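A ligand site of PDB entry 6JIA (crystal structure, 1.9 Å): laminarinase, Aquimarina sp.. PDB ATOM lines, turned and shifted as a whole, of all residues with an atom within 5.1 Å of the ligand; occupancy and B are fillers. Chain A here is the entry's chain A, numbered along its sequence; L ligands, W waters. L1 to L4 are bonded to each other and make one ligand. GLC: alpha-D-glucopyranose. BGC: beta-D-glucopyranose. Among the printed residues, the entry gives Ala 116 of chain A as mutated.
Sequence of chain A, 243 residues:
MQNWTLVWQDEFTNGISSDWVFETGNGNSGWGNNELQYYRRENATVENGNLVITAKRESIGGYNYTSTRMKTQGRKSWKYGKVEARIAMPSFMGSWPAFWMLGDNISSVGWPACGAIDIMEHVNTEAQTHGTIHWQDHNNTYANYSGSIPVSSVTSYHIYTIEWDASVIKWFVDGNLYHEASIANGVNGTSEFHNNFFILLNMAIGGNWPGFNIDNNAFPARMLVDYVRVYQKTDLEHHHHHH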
ATOM      1  N   TRP A  31     -16.552   6.239 -31.049  1.00  0.00           N
ATOM      2  CA  TRP A  31     -16.458   5.862 -29.620  1.00  0.00           C
ATOM      3  C   TRP A  31     -17.329   4.643 -29.368  1.00  0.00           C
ATOM      4  O   TRP A  31     -17.862   4.516 -28.251  1.00  0.00           O
ATOM      5  CB  TRP A  31     -16.805   7.060 -28.730  1.00  0.00           C
ATOM      6  CG  TRP A  31     -15.764   8.127 -28.866  1.00  0.00           C
ATOM      7  CD1 TRP A  31     -15.778   9.153 -29.756  1.00  0.00           C
ATOM      8  CD2 TRP A  31     -14.472   8.140 -28.243  1.00  0.00           C
ATOM      9  NE1 TRP A  31     -14.617   9.842 -29.692  1.00  0.00           N
ATOM     10  CE2 TRP A  31     -13.777   9.242 -28.773  1.00  0.00           C
ATOM     11  CE3 TRP A  31     -13.821   7.340 -27.292  1.00  0.00           C
ATOM     12  CZ2 TRP A  31     -12.469   9.574 -28.386  1.00  0.00           C
ATOM     13  CZ3 TRP A  31     -12.540   7.680 -26.881  1.00  0.00           C
ATOM     14  CH2 TRP A  31     -11.861   8.773 -27.448  1.00  0.00           C
ATOM     15  N   GLY A  32     -17.383   3.748 -30.353  1.00  0.00           N
ATOM     16  CA  GLY A  32     -18.132   2.485 -30.280  1.00  0.00           C
ATOM     17  C   GLY A  32     -19.644   2.615 -30.488  1.00  0.00           C
ATOM     18  O   GLY A  32     -20.304   1.586 -30.422  1.00  0.00           O
ATOM     19  N   ASN A  33     -20.149   3.791 -30.812  1.00  0.00           N
ATOM     20  CA  ASN A  33     -21.613   4.077 -30.896  1.00  0.00           C
ATOM     21  C   ASN A  33     -21.943   4.832 -32.186  1.00  0.00           C
ATOM     22  O   ASN A  33     -23.050   5.363 -32.288  1.00  0.00           O
ATOM     23  CB  ASN A  33     -22.101   4.884 -29.694  1.00  0.00           C
ATOM     24  CG  ASN A  33     -21.739   4.274 -28.354  1.00  0.00           C
ATOM     25  OD1 ASN A  33     -21.256   4.972 -27.434  1.00  0.00           O
ATOM     26  ND2 ASN A  33     -22.015   2.996 -28.206  1.00  0.00           N
ATOM     27  N   GLU A  35     -20.927   7.668 -33.078  1.00  0.00           N
ATOM     28  CA  GLU A  35     -21.108   9.123 -32.762  1.00  0.00           C
ATOM     29  C   GLU A  35     -20.439   9.957 -33.843  1.00  0.00           C
ATOM     30  O   GLU A  35     -19.513   9.457 -34.503  1.00  0.00           O
ATOM     31  CB  GLU A  35     -20.504   9.467 -31.415  1.00  0.00           C
ATOM     32  CG  GLU A  35     -21.079   8.606 -30.317  1.00  0.00           C
ATOM     33  CD  GLU A  35     -20.309   8.587 -29.034  1.00  0.00           C
ATOM     34  OE1 GLU A  35     -19.328   9.392 -28.914  1.00  0.00           O
ATOM     35  OE2 GLU A  35     -20.666   7.741 -28.177  1.00  0.00           O
ATOM     36  N   ARG A  69     -14.711  15.285 -24.324  1.00  0.00           N
ATOM     37  CA  ARG A  69     -14.813  14.117 -23.425  1.00  0.00           C
ATOM     38  C   ARG A  69     -13.630  14.202 -22.482  1.00  0.00           C
ATOM     39  O   ARG A  69     -12.512  14.172 -22.961  1.00  0.00           O
ATOM     40  CB  ARG A  69     -14.817  12.827 -24.260  1.00  0.00           C
ATOM     41  CG  ARG A  69     -14.791  11.553 -23.433  1.00  0.00           C
ATOM     42  CD  ARG A  69     -15.166  10.428 -24.355  1.00  0.00           C
ATOM     43  NE  ARG A  69     -14.831   9.112 -23.863  1.00  0.00           N
ATOM     44  CZ  ARG A  69     -15.447   7.968 -24.184  1.00  0.00           C
ATOM     45  NH1 ARG A  69     -16.487   7.946 -24.989  1.00  0.00           N
ATOM     46  NH2 ARG A  69     -15.018   6.854 -23.650  1.00  0.00           N
ATOM     47  N   TRP A  96     -26.300  14.152 -26.822  1.00  0.00           N
ATOM     48  CA  TRP A  96     -26.132  12.970 -25.934  1.00  0.00           C
ATOM     49  C   TRP A  96     -25.079  13.262 -24.871  1.00  0.00           C
ATOM     50  O   TRP A  96     -23.935  12.847 -24.974  1.00  0.00           O
ATOM     51  CB  TRP A  96     -25.854  11.751 -26.794  1.00  0.00           C
ATOM     52  CG  TRP A  96     -25.703  10.481 -26.023  1.00  0.00           C
ATOM     53  CD1 TRP A  96     -26.093  10.208 -24.745  1.00  0.00           C
ATOM     54  CD2 TRP A  96     -25.129   9.280 -26.527  1.00  0.00           C
ATOM     55  NE1 TRP A  96     -25.780   8.924 -24.406  1.00  0.00           N
ATOM     56  CE2 TRP A  96     -25.186   8.330 -25.479  1.00  0.00           C
ATOM     57  CE3 TRP A  96     -24.603   8.905 -27.764  1.00  0.00           C
ATOM     58  CZ2 TRP A  96     -24.725   7.020 -25.660  1.00  0.00           C
ATOM     59  CZ3 TRP A  96     -24.149   7.628 -27.923  1.00  0.00           C
ATOM     60  CH2 TRP A  96     -24.186   6.705 -26.878  1.00  0.00           C
ATOM     61  N   ALA A  98     -23.360  13.044 -21.096  1.00  0.00           N
ATOM     62  CA  ALA A  98     -23.221  11.949 -20.126  1.00  0.00           C
ATOM     63  C   ALA A  98     -22.280  12.361 -18.999  1.00  0.00           C
ATOM     64  O   ALA A  98     -21.293  13.094 -19.206  1.00  0.00           O
ATOM     65  CB  ALA A  98     -22.771  10.698 -20.826  1.00  0.00           C
ATOM     66  N   TRP A 100     -20.593   9.826 -16.153  1.00  0.00           N
ATOM     67  CA  TRP A 100     -20.460   8.363 -16.010  1.00  0.00           C
ATOM     68  C   TRP A 100     -19.086   7.960 -15.482  1.00  0.00           C
ATOM     69  O   TRP A 100     -18.223   8.824 -15.200  1.00  0.00           O
ATOM     70  CB  TRP A 100     -20.788   7.680 -17.331  1.00  0.00           C
ATOM     71  CG  TRP A 100     -19.996   8.089 -18.536  1.00  0.00           C
ATOM     72  CD1 TRP A 100     -19.908   9.326 -19.130  1.00  0.00           C
ATOM     73  CD2 TRP A 100     -19.297   7.184 -19.402  1.00  0.00           C
ATOM     74  NE1 TRP A 100     -19.173   9.250 -20.277  1.00  0.00           N
ATOM     75  CE2 TRP A 100     -18.817   7.947 -20.495  1.00  0.00           C
ATOM     76  CE3 TRP A 100     -19.123   5.803 -19.413  1.00  0.00           C
ATOM     77  CZ2 TRP A 100     -18.124   7.360 -21.556  1.00  0.00           C
ATOM     78  CZ3 TRP A 100     -18.403   5.228 -20.450  1.00  0.00           C
ATOM     79  CH2 TRP A 100     -17.920   6.003 -21.502  1.00  0.00           C
ATOM     80  N   LEU A 102     -16.152   4.434 -15.528  1.00  0.00           N
ATOM     81  CA  LEU A 102     -15.578   3.197 -16.111  1.00  0.00           C
ATOM     82  C   LEU A 102     -14.625   2.570 -15.086  1.00  0.00           C
ATOM     83  O   LEU A 102     -13.869   3.309 -14.419  1.00  0.00           O
ATOM     84  CB  LEU A 102     -14.823   3.533 -17.395  1.00  0.00           C
ATOM     85  CG  LEU A 102     -15.663   3.760 -18.645  1.00  0.00           C
ATOM     86  CD1 LEU A 102     -14.760   4.294 -19.785  1.00  0.00           C
ATOM     87  CD2 LEU A 102     -16.385   2.483 -19.073  1.00  0.00           C
ATOM     88  N   ILE A 106     -10.256  -1.122 -17.472  1.00  0.00           N
ATOM     89  CA  ILE A 106     -10.606  -1.131 -18.910  1.00  0.00           C
ATOM     90  C   ILE A 106      -9.334  -1.290 -19.766  1.00  0.00           C
ATOM     91  O   ILE A 106      -9.450  -1.855 -20.876  1.00  0.00           O
ATOM     92  CB  ILE A 106     -11.380   0.124 -19.292  1.00  0.00           C
ATOM     93  CG1 ILE A 106     -11.912   0.007 -20.706  1.00  0.00           C
ATOM     94  CG2 ILE A 106     -10.506   1.368 -19.091  1.00  0.00           C
ATOM     95  CD1 ILE A 106     -12.873   1.123 -21.081  1.00  0.00           C
ATOM     96  N   TRP A 111     -14.032  -2.880 -22.384  1.00  0.00           N
ATOM     97  CA  TRP A 111     -15.488  -2.715 -22.149  1.00  0.00           C
ATOM     98  C   TRP A 111     -16.207  -3.874 -22.866  1.00  0.00           C
ATOM     99  O   TRP A 111     -15.837  -4.221 -23.985  1.00  0.00           O
ATOM    100  CB  TRP A 111     -15.905  -1.331 -22.686  1.00  0.00           C
ATOM    101  CG  TRP A 111     -17.331  -0.994 -22.420  1.00  0.00           C
ATOM    102  CD1 TRP A 111     -17.832  -0.190 -21.430  1.00  0.00           C
ATOM    103  CD2 TRP A 111     -18.471  -1.485 -23.147  1.00  0.00           C
ATOM    104  NE1 TRP A 111     -19.195  -0.130 -21.518  1.00  0.00           N
ATOM    105  CE2 TRP A 111     -19.619  -0.887 -22.571  1.00  0.00           C
ATOM    106  CE3 TRP A 111     -18.613  -2.271 -24.294  1.00  0.00           C
ATOM    107  CZ2 TRP A 111     -20.888  -1.118 -23.065  1.00  0.00           C
ATOM    108  CZ3 TRP A 111     -19.881  -2.526 -24.755  1.00  0.00           C
ATOM    109  CH2 TRP A 111     -20.992  -1.935 -24.158  1.00  0.00           C
ATOM    110  N   ALA A 116     -19.428  -0.146 -16.437  1.00  0.00           N
ATOM    111  CA  ALA A 116     -19.729   1.287 -16.539  1.00  0.00           C
ATOM    112  C   ALA A 116     -20.922   1.612 -15.644  1.00  0.00           C
ATOM    113  O   ALA A 116     -21.880   0.818 -15.611  1.00  0.00           O
ATOM    114  CB  ALA A 116     -19.998   1.631 -17.986  1.00  0.00           C
ATOM    115  N   ASP A 118     -23.373   4.733 -15.561  1.00  0.00           N
ATOM    116  CA  ASP A 118     -23.864   6.022 -16.084  1.00  0.00           C
ATOM    117  C   ASP A 118     -24.680   6.707 -14.992  1.00  0.00           C
ATOM    118  O   ASP A 118     -25.757   6.211 -14.637  1.00  0.00           O
ATOM    119  CB  ASP A 118     -24.688   5.866 -17.358  1.00  0.00           C
ATOM    120  CG  ASP A 118     -23.831   5.467 -18.546  1.00  0.00           C
ATOM    121  OD1 ASP A 118     -23.629   4.275 -18.682  1.00  0.00           O
ATOM    122  OD2 ASP A 118     -23.365   6.401 -19.324  1.00  0.00           O
ATOM    123  N   GLU A 121     -27.415  10.177 -18.127  1.00  0.00           N
ATOM    124  CA  GLU A 121     -27.435  10.358 -19.583  1.00  0.00           C
ATOM    125  C   GLU A 121     -28.746  10.993 -20.007  1.00  0.00           C
ATOM    126  O   GLU A 121     -29.784  10.742 -19.415  1.00  0.00           O
ATOM    127  CB  GLU A 121     -27.277   9.037 -20.325  1.00  0.00           C
ATOM    128  CG  GLU A 121     -25.911   8.425 -20.152  1.00  0.00           C
ATOM    129  CD  GLU A 121     -25.797   7.122 -20.895  1.00  0.00           C
ATOM    130  OE1 GLU A 121     -26.332   6.080 -20.339  1.00  0.00           O
ATOM    131  OE2 GLU A 121     -25.351   7.182 -22.063  1.00  0.00           O
ATOM    132  N   HIS A 134     -23.668  -1.051 -16.962  1.00  0.00           N
ATOM    133  CA  HIS A 134     -23.280  -1.933 -18.085  1.00  0.00           C
ATOM    134  C   HIS A 134     -22.178  -2.855 -17.602  1.00  0.00           C
ATOM    135  O   HIS A 134     -21.270  -2.350 -16.981  1.00  0.00           O
ATOM    136  CB  HIS A 134     -22.740  -1.127 -19.265  1.00  0.00           C
ATOM    137  CG  HIS A 134     -23.684  -0.133 -19.833  1.00  0.00           C
ATOM    138  ND1 HIS A 134     -24.388  -0.391 -20.985  1.00  0.00           N
ATOM    139  CD2 HIS A 134     -23.967   1.153 -19.479  1.00  0.00           C
ATOM    140  CE1 HIS A 134     -25.084   0.677 -21.330  1.00  0.00           C
ATOM    141  NE2 HIS A 134     -24.856   1.634 -20.405  1.00  0.00           N
ATOM    142  N   TYR A 142     -23.119  -9.443 -22.499  1.00  0.00           N
ATOM    143  CA  TYR A 142     -23.218  -7.987 -22.253  1.00  0.00           C
ATOM    144  C   TYR A 142     -24.599  -7.758 -21.634  1.00  0.00           C
ATOM    145  O   TYR A 142     -25.606  -8.277 -22.165  1.00  0.00           O
ATOM    146  CB  TYR A 142     -22.976  -7.213 -23.547  1.00  0.00           C
ATOM    147  CG  TYR A 142     -23.427  -5.791 -23.436  1.00  0.00           C
ATOM    148  CD1 TYR A 142     -23.001  -4.995 -22.397  1.00  0.00           C
ATOM    149  CD2 TYR A 142     -24.333  -5.259 -24.351  1.00  0.00           C
ATOM    150  CE1 TYR A 142     -23.463  -3.702 -22.251  1.00  0.00           C
ATOM    151  CE2 TYR A 142     -24.825  -3.972 -24.200  1.00  0.00           C
ATOM    152  CZ  TYR A 142     -24.391  -3.194 -23.150  1.00  0.00           C
ATOM    153  OH  TYR A 142     -24.833  -1.917 -22.983  1.00  0.00           O
ATOM    154  N   ASN A 202     -18.959  14.027 -20.830  1.00  0.00           N
ATOM    155  CA  ASN A 202     -18.874  14.350 -22.268  1.00  0.00           C
ATOM    156  C   ASN A 202     -20.215  14.835 -22.771  1.00  0.00           C
ATOM    157  O   ASN A 202     -21.212  14.710 -22.058  1.00  0.00           O
ATOM    158  CB  ASN A 202     -18.405  13.132 -23.073  1.00  0.00           C
ATOM    159  CG  ASN A 202     -19.452  12.045 -23.101  1.00  0.00           C
ATOM    160  OD1 ASN A 202     -19.586  11.263 -22.138  1.00  0.00           O
ATOM    161  ND2 ASN A 202     -20.206  11.998 -24.188  1.00  0.00           N
HETATM  162  C1  GLC L   1     -22.566   4.080 -21.611  1.00  0.00           C
HETATM  163  C2  GLC L   1     -22.214   3.489 -22.972  1.00  0.00           C
HETATM  164  C3  GLC L   1     -21.001   4.130 -23.566  1.00  0.00           C
HETATM  165  C4  GLC L   1     -21.201   5.608 -23.670  1.00  0.00           C
HETATM  166  C5  GLC L   1     -21.423   6.162 -22.213  1.00  0.00           C
HETATM  167  C6  GLC L   1     -21.730   7.680 -22.193  1.00  0.00           C
HETATM  168  O1  GLC L   1     -21.656   3.657 -20.599  1.00  0.00           O
HETATM  169  O2  GLC L   1     -22.185   2.114 -22.844  1.00  0.00           O
HETATM  170  O3  GLC L   1     -20.791   3.567 -24.872  1.00  0.00           O
HETATM  171  O4  GLC L   1     -20.124   6.230 -24.345  1.00  0.00           O
HETATM  172  O5  GLC L   1     -22.645   5.506 -21.755  1.00  0.00           O
HETATM  173  O6  GLC L   1     -22.857   8.026 -23.012  1.00  0.00           O
HETATM  174  C2  BGC L   2     -19.585   1.945 -26.337  1.00  0.00           C
HETATM  175  C3  BGC L   2     -18.509   0.890 -26.290  1.00  0.00           C
HETATM  176  C4  BGC L   2     -17.231   1.473 -25.691  1.00  0.00           C
HETATM  177  C5  BGC L   2     -17.508   2.066 -24.255  1.00  0.00           C
HETATM  178  C6  BGC L   2     -16.267   2.862 -23.677  1.00  0.00           C
HETATM  179  C1  BGC L   2     -19.795   2.496 -24.884  1.00  0.00           C
HETATM  180  O2  BGC L   2     -20.812   1.374 -26.670  1.00  0.00           O
HETATM  181  O3  BGC L   2     -18.333   0.519 -27.642  1.00  0.00           O
HETATM  182  O4  BGC L   2     -16.150   0.528 -25.547  1.00  0.00           O
HETATM  183  O5  BGC L   2     -18.577   3.071 -24.415  1.00  0.00           O
HETATM  184  O6  BGC L   2     -15.957   3.985 -24.576  1.00  0.00           O
HETATM  185  C2  BGC L   3     -18.436  -1.202 -29.253  1.00  0.00           C
HETATM  186  C3  BGC L   3     -18.243  -2.688 -29.460  1.00  0.00           C
HETATM  187  C4  BGC L   3     -16.845  -3.145 -29.064  1.00  0.00           C
HETATM  188  C5  BGC L   3     -16.644  -2.679 -27.584  1.00  0.00           C
HETATM  189  C6  BGC L   3     -15.296  -3.066 -26.873  1.00  0.00           C
HETATM  190  C1  BGC L   3     -18.147  -0.918 -27.772  1.00  0.00           C
HETATM  191  O2  BGC L   3     -19.742  -0.906 -29.471  1.00  0.00           O
HETATM  192  O3  BGC L   3     -18.415  -2.960 -30.885  1.00  0.00           O
HETATM  193  O4  BGC L   3     -16.818  -4.516 -29.242  1.00  0.00           O
HETATM  194  O5  BGC L   3     -16.757  -1.247 -27.501  1.00  0.00           O
HETATM  195  O6  BGC L   3     -14.308  -2.617 -27.812  1.00  0.00           O
HETATM  196  C2  BGC L   4     -19.910  -3.647 -32.669  1.00  0.00           C
HETATM  197  C3  BGC L   4     -21.045  -4.572 -33.007  1.00  0.00           C
HETATM  198  C4  BGC L   4     -20.859  -5.949 -32.473  1.00  0.00           C
HETATM  199  C5  BGC L   4     -20.447  -5.955 -30.966  1.00  0.00           C
HETATM  200  C6  BGC L   4     -20.044  -7.375 -30.446  1.00  0.00           C
HETATM  201  C1  BGC L   4     -19.598  -3.676 -31.172  1.00  0.00           C
HETATM  202  O2  BGC L   4     -20.248  -2.356 -33.056  1.00  0.00           O
HETATM  203  O3  BGC L   4     -21.189  -4.650 -34.375  1.00  0.00           O
HETATM  204  O4  BGC L   4     -22.046  -6.665 -32.652  1.00  0.00           O
HETATM  205  O5  BGC L   4     -19.283  -5.050 -30.802  1.00  0.00           O
HETATM  206  O6  BGC L   4     -18.647  -7.618 -30.697  1.00  0.00           O
HETATM  207  O   HOH W   1     -13.145   0.795 -24.728  1.00  0.00           O
HETATM  208  O   HOH W   2     -18.065  -9.960 -29.131  1.00  0.00           O
HETATM  209  O   HOH W   3     -21.930   0.498 -32.863  1.00  0.00           O
HETATM  210  O   HOH W   4     -20.708   8.391 -25.646  1.00  0.00           O
HETATM  211  O   HOH W   5     -22.383  -1.773 -31.778  1.00  0.00           O
HETATM  212  O   HOH W   6     -23.313   1.189 -25.116  1.00  0.00           O
HETATM  213  O   HOH W   7     -17.892   5.544 -25.780  1.00  0.00           O
HETATM  214  O   HOH W   8     -13.337   3.740 -25.746  1.00  0.00           O
HETATM  215  O   HOH W   9     -21.988  -1.775 -28.107  1.00  0.00           O
HETATM  216  O   HOH W  10     -22.610  10.264 -24.474  1.00  0.00           O
HETATM  217  O   HOH W  11     -25.503   4.516 -23.207  1.00  0.00           O
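Water W4 lies within hydrogen-bond range of an oxygen (O4) of GLC L1 (2.6 Å) and the side-chain carboxylate of Glu 35 (2.6 Å). Water W10 lies within hydrogen-bond range of an oxygen (O6) of GLC L1, the backbone carbonyl oxygen of Trp 96 and the side-chain amide nitrogen of Asn 202. Water W7 lies within hydrogen-bond range of O of Trp 31 (2.7 Å), O4 of GLC L1 (2.7 Å) and NH1 of Arg 69 (2.9 Å). Water W3 bridges O of Gly 32 and O2 of BGC L4. Water W11 lies within hydrogen-bond range of the side-chain carboxylate of Glu 121 and an oxygen (O5) of GLC L1.
The indole nitrogen of Trp 96 sits at hydrogen-bond distance from an oxygen (O6) of GLC L1 (3.4 Å). The side-chain amide nitrogen (ND2) of Asn 33 sits at hydrogen-bond distance from an oxygen (O2) of BGC L2 (2.5 Å). The guanidinium group of Arg 69 is in hydrogen-bond range of an oxygen (O6) of BGC L2 (3.2 Å). The backbone carbonyl oxygen of Gly 32 is in hydrogen-bond range of an oxygen (O2) of BGC L3. O6 of GLC L1 is in hydrogen-bond range of OE2 of Glu 121, 2.8 Å away. OD1 of Asp 118 is in hydrogen-bond range of O1 of GLC L1 (2.8 Å).
Merely in contact with the ligand: Trp 31, Ala 98, Trp 100, Trp 111, Ala 116 and His 134. Hydrophobic or aromatic side chains within 4 Å of the ligand: Trp 96, Ala 98, Trp 100, Trp 111, Ala 116 and His 134. Of the 17 residues printed, 12 come within 4 Å of the ligand. The nearest printed residue that does not touch the ligand is Glu 35 (4.2 Å).
The side-chain carboxylate (OE2) of Glu 121 lies within hydrogen-bond range of the indole nitrogen (NE1) of Trp 96, 3.0 Å away. NE1 of Trp 100 lies within hydrogen-bond range of OD1 of Asn 202 (2.8 Å). The side-chain carboxylate of Asp 118 sits close to a ring nitrogen (NE2) of His 134 (3.4 Å). The backbone carbonyl oxygen (O) of Asn 202 sits at hydrogen-bond distance from the backbone NH (N) of Ala 98, 2.9 Å away. The side-chain hydroxyl (OH) of Tyr 142 sits at hydrogen-bond distance from a ring nitrogen (ND1) of His 134, 2.6 Å away. OD1 of Asn 33 sits close to OE2 of Glu 35, at 2.9 Å. The backbone carbonyl oxygen (O) of Ala 116 lies within hydrogen-bond range of the backbone NH (N) of His 134 (2.9 Å).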
